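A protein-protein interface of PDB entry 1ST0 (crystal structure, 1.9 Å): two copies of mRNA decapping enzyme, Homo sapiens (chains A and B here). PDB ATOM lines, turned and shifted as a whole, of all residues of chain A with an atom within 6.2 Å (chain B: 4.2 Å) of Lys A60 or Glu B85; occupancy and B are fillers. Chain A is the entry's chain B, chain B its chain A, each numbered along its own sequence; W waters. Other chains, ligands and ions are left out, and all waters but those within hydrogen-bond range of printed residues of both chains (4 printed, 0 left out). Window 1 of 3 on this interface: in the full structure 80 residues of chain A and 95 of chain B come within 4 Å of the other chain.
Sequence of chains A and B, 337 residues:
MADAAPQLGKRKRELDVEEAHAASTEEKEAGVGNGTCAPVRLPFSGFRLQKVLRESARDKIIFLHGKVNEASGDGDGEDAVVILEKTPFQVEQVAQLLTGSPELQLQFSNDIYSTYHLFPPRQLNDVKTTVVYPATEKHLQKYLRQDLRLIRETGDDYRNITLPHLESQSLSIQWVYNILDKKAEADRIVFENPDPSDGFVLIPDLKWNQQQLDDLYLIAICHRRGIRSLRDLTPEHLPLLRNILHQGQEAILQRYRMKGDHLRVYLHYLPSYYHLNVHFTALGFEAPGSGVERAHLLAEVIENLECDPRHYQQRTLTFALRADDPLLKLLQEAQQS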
ATOM      1  N   SER A  56      11.460  24.171 -11.305  1.00  0.00           N
ATOM      2  CA  SER A  56      11.092  24.120 -12.694  1.00  0.00           C
ATOM      3  C   SER A  56      11.803  22.940 -13.269  1.00  0.00           C
ATOM      4  O   SER A  56      13.073  22.908 -13.319  1.00  0.00           O
ATOM      5  CB  SER A  56      11.457  25.380 -13.453  1.00  0.00           C
ATOM      6  OG  SER A  56      11.232  25.146 -14.871  1.00  0.00           O
ATOM      7  N   ALA A  57      11.020  21.933 -13.644  1.00  0.00           N
ATOM      8  CA  ALA A  57      11.599  20.756 -14.294  1.00  0.00           C
ATOM      9  C   ALA A  57      11.965  21.071 -15.734  1.00  0.00           C
ATOM     10  O   ALA A  57      12.737  20.308 -16.343  1.00  0.00           O
ATOM     11  CB  ALA A  57      10.633  19.552 -14.235  1.00  0.00           C
ATOM     12  N   ARG A  58      11.472  22.177 -16.310  1.00  0.00           N
ATOM     13  CA  ARG A  58      11.897  22.566 -17.630  1.00  0.00           C
ATOM     14  C   ARG A  58      13.305  23.240 -17.545  1.00  0.00           C
ATOM     15  O   ARG A  58      14.210  22.961 -18.363  1.00  0.00           O
ATOM     16  CB  ARG A  58      10.925  23.579 -18.259  1.00  0.00           C
ATOM     17  CG  ARG A  58      11.399  24.113 -19.632  1.00  0.00           C
ATOM     18  CD  ARG A  58      11.469  22.952 -20.790  1.00  0.00           C
ATOM     19  NE  ARG A  58      11.919  23.519 -22.073  1.00  0.00           N
ATOM     20  CZ  ARG A  58      11.226  24.373 -22.805  1.00  0.00           C
ATOM     21  NH1 ARG A  58       9.970  24.697 -22.477  1.00  0.00           N
ATOM     22  NH2 ARG A  58      11.757  24.862 -23.902  1.00  0.00           N
ATOM     23  N   ASP A  59      13.475  24.123 -16.544  1.00  0.00           N
ATOM     24  CA  ASP A  59      14.726  24.885 -16.439  1.00  0.00           C
ATOM     25  C   ASP A  59      15.782  24.147 -15.646  1.00  0.00           C
ATOM     26  O   ASP A  59      16.932  24.608 -15.559  1.00  0.00           O
ATOM     27  CB  ASP A  59      14.428  26.209 -15.714  1.00  0.00           C
ATOM     28  CG  ASP A  59      13.567  27.151 -16.569  1.00  0.00           C
ATOM     29  OD1 ASP A  59      13.350  26.932 -17.792  1.00  0.00           O
ATOM     30  OD2 ASP A  59      13.022  28.150 -16.094  1.00  0.00           O
ATOM     31  N   LYS A  60      15.397  23.043 -15.034  1.00  0.00           N
ATOM     32  CA  LYS A  60      16.248  22.139 -14.254  1.00  0.00           C
ATOM     33  C   LYS A  60      16.825  22.964 -13.057  1.00  0.00           C
ATOM     34  O   LYS A  60      18.059  22.981 -12.806  1.00  0.00           O
ATOM     35  CB  LYS A  60      17.365  21.517 -15.082  1.00  0.00           C
ATOM     36  CG  LYS A  60      17.019  21.137 -16.575  1.00  0.00           C
ATOM     37  CD  LYS A  60      16.136  19.907 -16.466  1.00  0.00           C
ATOM     38  CE  LYS A  60      15.373  19.582 -17.732  1.00  0.00           C
ATOM     39  NZ  LYS A  60      15.849  20.209 -18.948  1.00  0.00           N
ATOM     40  N   ILE A  61      15.918  23.558 -12.300  1.00  0.00           N
ATOM     41  CA  ILE A  61      16.318  24.317 -11.110  1.00  0.00           C
ATOM     42  C   ILE A  61      15.387  24.041  -9.967  1.00  0.00           C
ATOM     43  O   ILE A  61      14.149  23.845 -10.207  1.00  0.00           O
ATOM     44  CB  ILE A  61      16.327  25.806 -11.506  1.00  0.00           C
ATOM     45  CG1 ILE A  61      16.962  26.727 -10.423  1.00  0.00           C
ATOM     46  CG2 ILE A  61      14.929  26.322 -11.975  1.00  0.00           C
ATOM     47  CD1 ILE A  61      17.148  28.183 -11.068  1.00  0.00           C
ATOM     48  N   ILE A  62      15.904  24.054  -8.747  1.00  0.00           N
ATOM     49  CA  ILE A  62      15.004  23.974  -7.579  1.00  0.00           C
ATOM     50  C   ILE A  62      15.477  24.950  -6.504  1.00  0.00           C
ATOM     51  O   ILE A  62      16.695  25.171  -6.400  1.00  0.00           O
ATOM     52  CB  ILE A  62      15.093  22.627  -6.925  1.00  0.00           C
ATOM     53  CG1 ILE A  62      16.548  22.273  -6.808  1.00  0.00           C
ATOM     54  CG2 ILE A  62      14.382  21.584  -7.726  1.00  0.00           C
ATOM     55  CD1 ILE A  62      16.768  20.998  -6.255  1.00  0.00           C
ATOM     56  N   LEU A  84      19.567  25.254  -6.694  1.00  0.00           N
ATOM     57  CA  LEU A  84      20.475  24.470  -7.496  1.00  0.00           C
ATOM     58  C   LEU A  84      20.007  24.404  -8.884  1.00  0.00           C
ATOM     59  O   LEU A  84      18.780  24.248  -9.173  1.00  0.00           O
ATOM     60  CB  LEU A  84      20.660  23.061  -6.981  1.00  0.00           C
ATOM     61  CG  LEU A  84      20.820  22.469  -5.589  1.00  0.00           C
ATOM     62  CD1 LEU A  84      22.158  21.956  -5.178  1.00  0.00           C
ATOM     63  CD2 LEU A  84      19.991  23.126  -4.503  1.00  0.00           C
ATOM     64  N   GLU A  85      20.954  24.526  -9.793  1.00  0.00           N
ATOM     65  CA  GLU A  85      20.602  24.607 -11.183  1.00  0.00           C
ATOM     66  C   GLU A  85      21.589  23.749 -11.942  1.00  0.00           C
ATOM     67  O   GLU A  85      22.852  23.904 -11.773  1.00  0.00           O
ATOM     68  CB  GLU A  85      20.543  26.057 -11.679  1.00  0.00           C
ATOM     69  CG  GLU A  85      20.113  26.211 -13.164  1.00  0.00           C
ATOM     70  CD  GLU A  85      20.079  27.643 -13.581  1.00  0.00           C
ATOM     71  OE1 GLU A  85      20.546  28.517 -12.786  1.00  0.00           O
ATOM     72  OE2 GLU A  85      19.543  27.926 -14.660  1.00  0.00           O
ATOM     73  N   LYS A  86      21.054  22.855 -12.804  1.00  0.00           N
ATOM     74  CA  LYS A  86      21.924  22.114 -13.765  1.00  0.00           C
ATOM     75  C   LYS A  86      22.660  23.080 -14.711  1.00  0.00           C
ATOM     76  O   LYS A  86      22.210  24.213 -14.964  1.00  0.00           O
ATOM     77  CB  LYS A  86      21.125  21.065 -14.577  1.00  0.00           C
ATOM     78  CG  LYS A  86      20.530  19.989 -13.518  1.00  0.00           C
ATOM     79  CD  LYS A  86      21.561  19.020 -13.014  1.00  0.00           C
ATOM     80  CE  LYS A  86      21.009  18.098 -11.948  1.00  0.00           C
ATOM     81  NZ  LYS A  86      20.243  16.920 -12.747  1.00  0.00           N
ATOM     82  N   PHE A  89      25.527  22.256 -21.489  1.00  0.00           N
ATOM     83  CA  PHE A  89      26.590  21.374 -22.003  1.00  0.00           C
ATOM     84  C   PHE A  89      27.703  22.216 -22.686  1.00  0.00           C
ATOM     85  O   PHE A  89      27.442  23.296 -23.217  1.00  0.00           O
ATOM     86  CB  PHE A  89      26.023  20.325 -23.012  1.00  0.00           C
ATOM     87  CG  PHE A  89      25.215  19.253 -22.328  1.00  0.00           C
ATOM     88  CD1 PHE A  89      23.839  19.335 -22.266  1.00  0.00           C
ATOM     89  CD2 PHE A  89      25.852  18.183 -21.721  1.00  0.00           C
ATOM     90  CE1 PHE A  89      23.104  18.337 -21.611  1.00  0.00           C
ATOM     91  CE2 PHE A  89      25.149  17.117 -21.059  1.00  0.00           C
ATOM     92  CZ  PHE A  89      23.747  17.217 -20.955  1.00  0.00           C
ATOM     93  N   ASP B  59      16.984  25.052 -21.110  1.00  0.00           N
ATOM     94  CA  ASP B  59      16.633  23.708 -20.592  1.00  0.00           C
ATOM     95  C   ASP B  59      17.840  22.758 -20.627  1.00  0.00           C
ATOM     96  O   ASP B  59      17.738  21.608 -20.206  1.00  0.00           O
ATOM     97  CB  ASP B  59      15.312  23.093 -21.201  1.00  0.00           C
ATOM     98  CG  ASP B  59      15.241  23.297 -22.652  1.00  0.00           C
ATOM     99  OD1 ASP B  59      14.262  22.868 -23.314  1.00  0.00           O
ATOM    100  OD2 ASP B  59      16.166  23.896 -23.214  1.00  0.00           O
ATOM    101  N   LYS B  60      19.021  23.305 -20.948  1.00  0.00           N
ATOM    102  CA  LYS B  60      20.313  22.585 -20.684  1.00  0.00           C
ATOM    103  C   LYS B  60      20.285  21.329 -21.557  1.00  0.00           C
ATOM    104  O   LYS B  60      20.400  20.171 -21.072  1.00  0.00           O
ATOM    105  CB  LYS B  60      20.528  22.165 -19.219  1.00  0.00           C
ATOM    106  CG  LYS B  60      20.869  23.356 -18.262  1.00  0.00           C
ATOM    107  CD  LYS B  60      19.574  24.107 -17.924  1.00  0.00           C
ATOM    108  CE  LYS B  60      19.889  25.248 -16.860  1.00  0.00           C
ATOM    109  NZ  LYS B  60      18.790  26.261 -16.760  1.00  0.00           N
ATOM    110  N   ILE B  61      20.141  21.589 -22.823  1.00  0.00           N
ATOM    111  CA  ILE B  61      19.989  20.503 -23.757  1.00  0.00           C
ATOM    112  C   ILE B  61      20.920  20.776 -24.925  1.00  0.00           C
ATOM    113  O   ILE B  61      21.239  21.954 -25.233  1.00  0.00           O
ATOM    114  CB  ILE B  61      18.545  20.436 -24.220  1.00  0.00           C
ATOM    115  CG1 ILE B  61      18.345  19.144 -25.103  1.00  0.00           C
ATOM    116  CG2 ILE B  61      18.115  21.744 -24.997  1.00  0.00           C
ATOM    117  CD1 ILE B  61      16.787  18.854 -25.303  1.00  0.00           C
ATOM    118  N   LEU B  84      21.341  15.258 -25.665  1.00  0.00           N
ATOM    119  CA  LEU B  84      21.639  15.132 -24.277  1.00  0.00           C
ATOM    120  C   LEU B  84      20.979  16.314 -23.542  1.00  0.00           C
ATOM    121  O   LEU B  84      21.034  17.473 -24.014  1.00  0.00           O
ATOM    122  CB  LEU B  84      23.171  15.207 -24.012  1.00  0.00           C
ATOM    123  CG  LEU B  84      24.097  14.187 -24.732  1.00  0.00           C
ATOM    124  CD1 LEU B  84      25.516  14.420 -24.268  1.00  0.00           C
ATOM    125  CD2 LEU B  84      23.814  12.822 -24.336  1.00  0.00           C
ATOM    126  N   GLU B  85      20.417  15.987 -22.381  1.00  0.00           N
ATOM    127  CA  GLU B  85      19.632  16.930 -21.616  1.00  0.00           C
ATOM    128  C   GLU B  85      19.919  16.638 -20.194  1.00  0.00           C
ATOM    129  O   GLU B  85      19.818  15.483 -19.706  1.00  0.00           O
ATOM    130  CB  GLU B  85      18.100  16.818 -21.992  1.00  0.00           C
ATOM    131  CG  GLU B  85      17.290  17.830 -21.225  1.00  0.00           C
ATOM    132  CD  GLU B  85      15.761  17.802 -21.568  1.00  0.00           C
ATOM    133  OE1 GLU B  85      15.012  18.743 -21.153  1.00  0.00           O
ATOM    134  OE2 GLU B  85      15.349  16.867 -22.305  1.00  0.00           O
ATOM    135  N   LYS B  86      20.252  17.697 -19.428  1.00  0.00           N
ATOM    136  CA  LYS B  86      20.434  17.517 -17.988  1.00  0.00           C
ATOM    137  C   LYS B  86      19.047  17.196 -17.378  1.00  0.00           C
ATOM    138  O   LYS B  86      18.066  17.623 -17.929  1.00  0.00           O
ATOM    139  CB  LYS B  86      20.942  18.826 -17.322  1.00  0.00           C
ATOM    140  CG  LYS B  86      22.406  19.214 -17.893  1.00  0.00           C
ATOM    141  CD  LYS B  86      23.385  18.185 -17.321  1.00  0.00           C
ATOM    142  CE  LYS B  86      24.828  18.362 -17.854  1.00  0.00           C
ATOM    143  NZ  LYS B  86      25.394  19.642 -17.233  1.00  0.00           N
ATOM    144  N   THR B  87      18.990  16.462 -16.269  1.00  0.00           N
ATOM    145  CA  THR B  87      17.670  16.050 -15.761  1.00  0.00           C
ATOM    146  C   THR B  87      17.189  16.971 -14.615  1.00  0.00           C
ATOM    147  O   THR B  87      17.952  17.742 -14.015  1.00  0.00           O
ATOM    148  CB  THR B  87      17.755  14.643 -15.241  1.00  0.00           C
ATOM    149  OG1 THR B  87      18.895  14.571 -14.348  1.00  0.00           O
ATOM    150  CG2 THR B  87      18.053  13.647 -16.441  1.00  0.00           C
ATOM    151  N   PRO B  88      15.896  16.911 -14.321  1.00  0.00           N
ATOM    152  CA  PRO B  88      15.344  17.668 -13.181  1.00  0.00           C
ATOM    153  C   PRO B  88      15.934  17.147 -11.909  1.00  0.00           C
ATOM    154  O   PRO B  88      16.338  16.002 -11.874  1.00  0.00           O
ATOM    155  CB  PRO B  88      13.850  17.244 -13.175  1.00  0.00           C
ATOM    156  CG  PRO B  88      13.598  16.868 -14.599  1.00  0.00           C
ATOM    157  CD  PRO B  88      14.855  16.161 -15.076  1.00  0.00           C
ATOM    158  N   PHE B  89      15.920  17.927 -10.839  1.00  0.00           N
ATOM    159  CA  PHE B  89      16.400  17.418  -9.614  1.00  0.00           C
ATOM    160  C   PHE B  89      15.357  16.524  -8.908  1.00  0.00           C
ATOM    161  O   PHE B  89      14.178  16.715  -9.080  1.00  0.00           O
ATOM    162  CB  PHE B  89      16.714  18.568  -8.692  1.00  0.00           C
ATOM    163  CG  PHE B  89      17.987  19.309  -9.081  1.00  0.00           C
ATOM    164  CD1 PHE B  89      17.923  20.451  -9.819  1.00  0.00           C
ATOM    165  CD2 PHE B  89      19.177  18.891  -8.601  1.00  0.00           C
ATOM    166  CE1 PHE B  89      19.144  21.171 -10.158  1.00  0.00           C
ATOM    167  CE2 PHE B  89      20.380  19.559  -8.942  1.00  0.00           C
ATOM    168  CZ  PHE B  89      20.342  20.676  -9.695  1.00  0.00           C
ATOM    169  N   VAL B 127      22.193  12.016 -17.150  1.00  0.00           N
ATOM    170  CA  VAL B 127      21.968  12.809 -18.307  1.00  0.00           C
ATOM    171  C   VAL B 127      21.001  12.021 -19.176  1.00  0.00           C
ATOM    172  O   VAL B 127      21.302  10.903 -19.598  1.00  0.00           O
ATOM    173  CB  VAL B 127      23.283  13.158 -19.084  1.00  0.00           C
ATOM    174  CG1 VAL B 127      23.032  13.662 -20.492  1.00  0.00           C
ATOM    175  CG2 VAL B 127      24.080  14.271 -18.263  1.00  0.00           C
ATOM    176  N   LYS B 128      19.940  12.700 -19.608  1.00  0.00           N
ATOM    177  CA  LYS B 128      18.936  11.982 -20.438  1.00  0.00           C
ATOM    178  C   LYS B 128      19.461  11.977 -21.892  1.00  0.00           C
ATOM    179  O   LYS B 128      19.757  13.049 -22.487  1.00  0.00           O
ATOM    180  CB  LYS B 128      17.581  12.731 -20.327  1.00  0.00           C
ATOM    181  CG  LYS B 128      16.425  12.026 -21.015  1.00  0.00           C
ATOM    182  CD  LYS B 128      15.105  12.823 -20.713  1.00  0.00           C
ATOM    183  CE  LYS B 128      15.085  14.168 -21.433  1.00  0.00           C
ATOM    184  NZ  LYS B 128      15.028  14.030 -22.939  1.00  0.00           N
HETATM  185  O   HOH W   1      21.909  15.957 -14.973  1.00  0.00           O
HETATM  186  O   HOH W   2      14.848  24.917 -25.219  1.00  0.00           O
HETATM  187  O   HOH W   3      14.489  20.397 -11.369  1.00  0.00           O
HETATM  188  O   HOH W   4      23.229  22.977 -23.098  1.00  0.00           O
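The guanidinium group (NE) of Arg A58 lies within salt-bridge range of the side-chain carboxylate (OD1) of Asp B59 (2.7 Å). The side-chain amino group (NZ) of Lys B60 lies within hydrogen-bond range of the backbone carbonyl oxygen (O) of Asp A59 (2.8 Å). The side-chain amino group (NZ) of Lys A60 is in hydrogen-bond range of the backbone carbonyl oxygen (O) of Asp B59 (2.7 Å). The side-chain amino group (NZ) of Lys A60 lies within salt-bridge range of the side-chain carboxylate (OE1) of Glu B85 (2.8 Å). The side-chain carboxylate (OE2) of Glu A85 lies within salt-bridge range of the side-chain amino group (NZ) of Lys B60, at 2.8 Å. NZ of Lys A86 lies within hydrogen-bond range of O of Thr B87 (2.7 Å).
The side-chain hydroxyl (OG) of Ser A56 sits close to the backbone NH (N) of Arg A58, 3.3 Å away. The backbone NH (N) of Asp A59 lies within hydrogen-bond range of the side-chain hydroxyl (OG) of Ser A56 (3.0 Å). The side-chain amino group (NZ) of Lys A60 lies within hydrogen-bond range of the backbone carbonyl oxygen (O) of Arg A58, at 3.3 Å. O of Ile A62 sits at hydrogen-bond distance from N of Leu A84 (2.9 Å). N of Lys B86 sits at hydrogen-bond distance from O of Lys B60 (3.0 Å). The side-chain carboxylate (OE2) of Glu B85 lies within salt-bridge range of the side-chain amino group (NZ) of Lys B128, at 2.9 Å.
Pro B88 touches Ala A57 (CG to O, 3.95 Å). Lys A60 touches Thr B87. O of Lys A60 touches CE1 of Phe B89, at 3.4 Å. CD1 of Ile A62 touches CB of Phe B89 (3.4 Å). Leu A84 touches Phe B89. CE1 of Phe B89 touches N of Glu A85, 3.8 Å away. CE1 of Phe A89 touches O of Leu B84 (3.3 Å). N of Glu B85 touches CE1 of Phe A89, 3.7 Å away. Phe A89 touches Lys B86. Phe A89 touches Val B127 (CZ to CG1, 3.7 Å).
Lys A60 touches just these residues of chain B: Asp B59 (2.7 Å), Glu B85 (2.8 Å), Lys B86 (3.3 Å), Thr B87 (3.6 Å), Pro B88 (3.7 Å) and Phe B89 (3.4 Å). Glu B85 touches just these residues of chain A: Lys A60 and Phe A89. Printed residues of chain B within 4 Å of Phe A89: Lys B60, Leu B84, Glu B85, Lys B86 and Val B127. Printed residues of chain A within 4 Å of Leu B84: Phe A89 (3.3 Å). Ser A56 touches none of the printed residues of chain B. Ile A61 touches none of the printed residues of chain B. The nearest residue of chain B that does not touch Lys A60 is Lys B60 (4.1 Å). The nearest printed residue of chain A that does not touch Lys B86 is Ala A57 (6.2 Å).
Of the 11 printed residues of chain A, 9 touch a printed residue of chain B. Hydrophobic or aromatic side chains of chain A within 4 Å of the printed part of chain B: Ile A62, Leu A84 and Phe A89. Among the printed residues, 22 pairs touch across the chains.
Lys A60 touches Glu B85, and with the chains exchanged Glu A85 touches Lys B60. Lys A60 touches Lys B86, and with the chains exchanged Lys A86 touches Lys B60. Lys A60 touches Phe B89, and with the chains exchanged Phe A89 touches Lys B60. Leu A84 touches Phe B89, and with the chains exchanged Phe A89 touches Leu B84. Positions printed for both chains: 59, 60, 61, 84, 85, 86 and 89. Of the 22 pairs that touch across the chains among the printed residues, 15 have their exchanged pair printed and touching as well.
Water W2 lies within hydrogen-bond range of the side-chain carboxylate of Asp B59 (2.6 Å) and the guanidinium group of Arg A58 (3.4 Å). Water W4 lies within hydrogen-bond range of N of Phe A89 (2.9 Å) and O of Ile B61 (3.1 Å). Water W3 lies within hydrogen-bond range of N of Phe B89 and O of Ser A56. Water W1 lies within hydrogen-bond range of the side-chain amino group (NZ) of Lys A86 and the backbone NH (N) of Thr B87.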
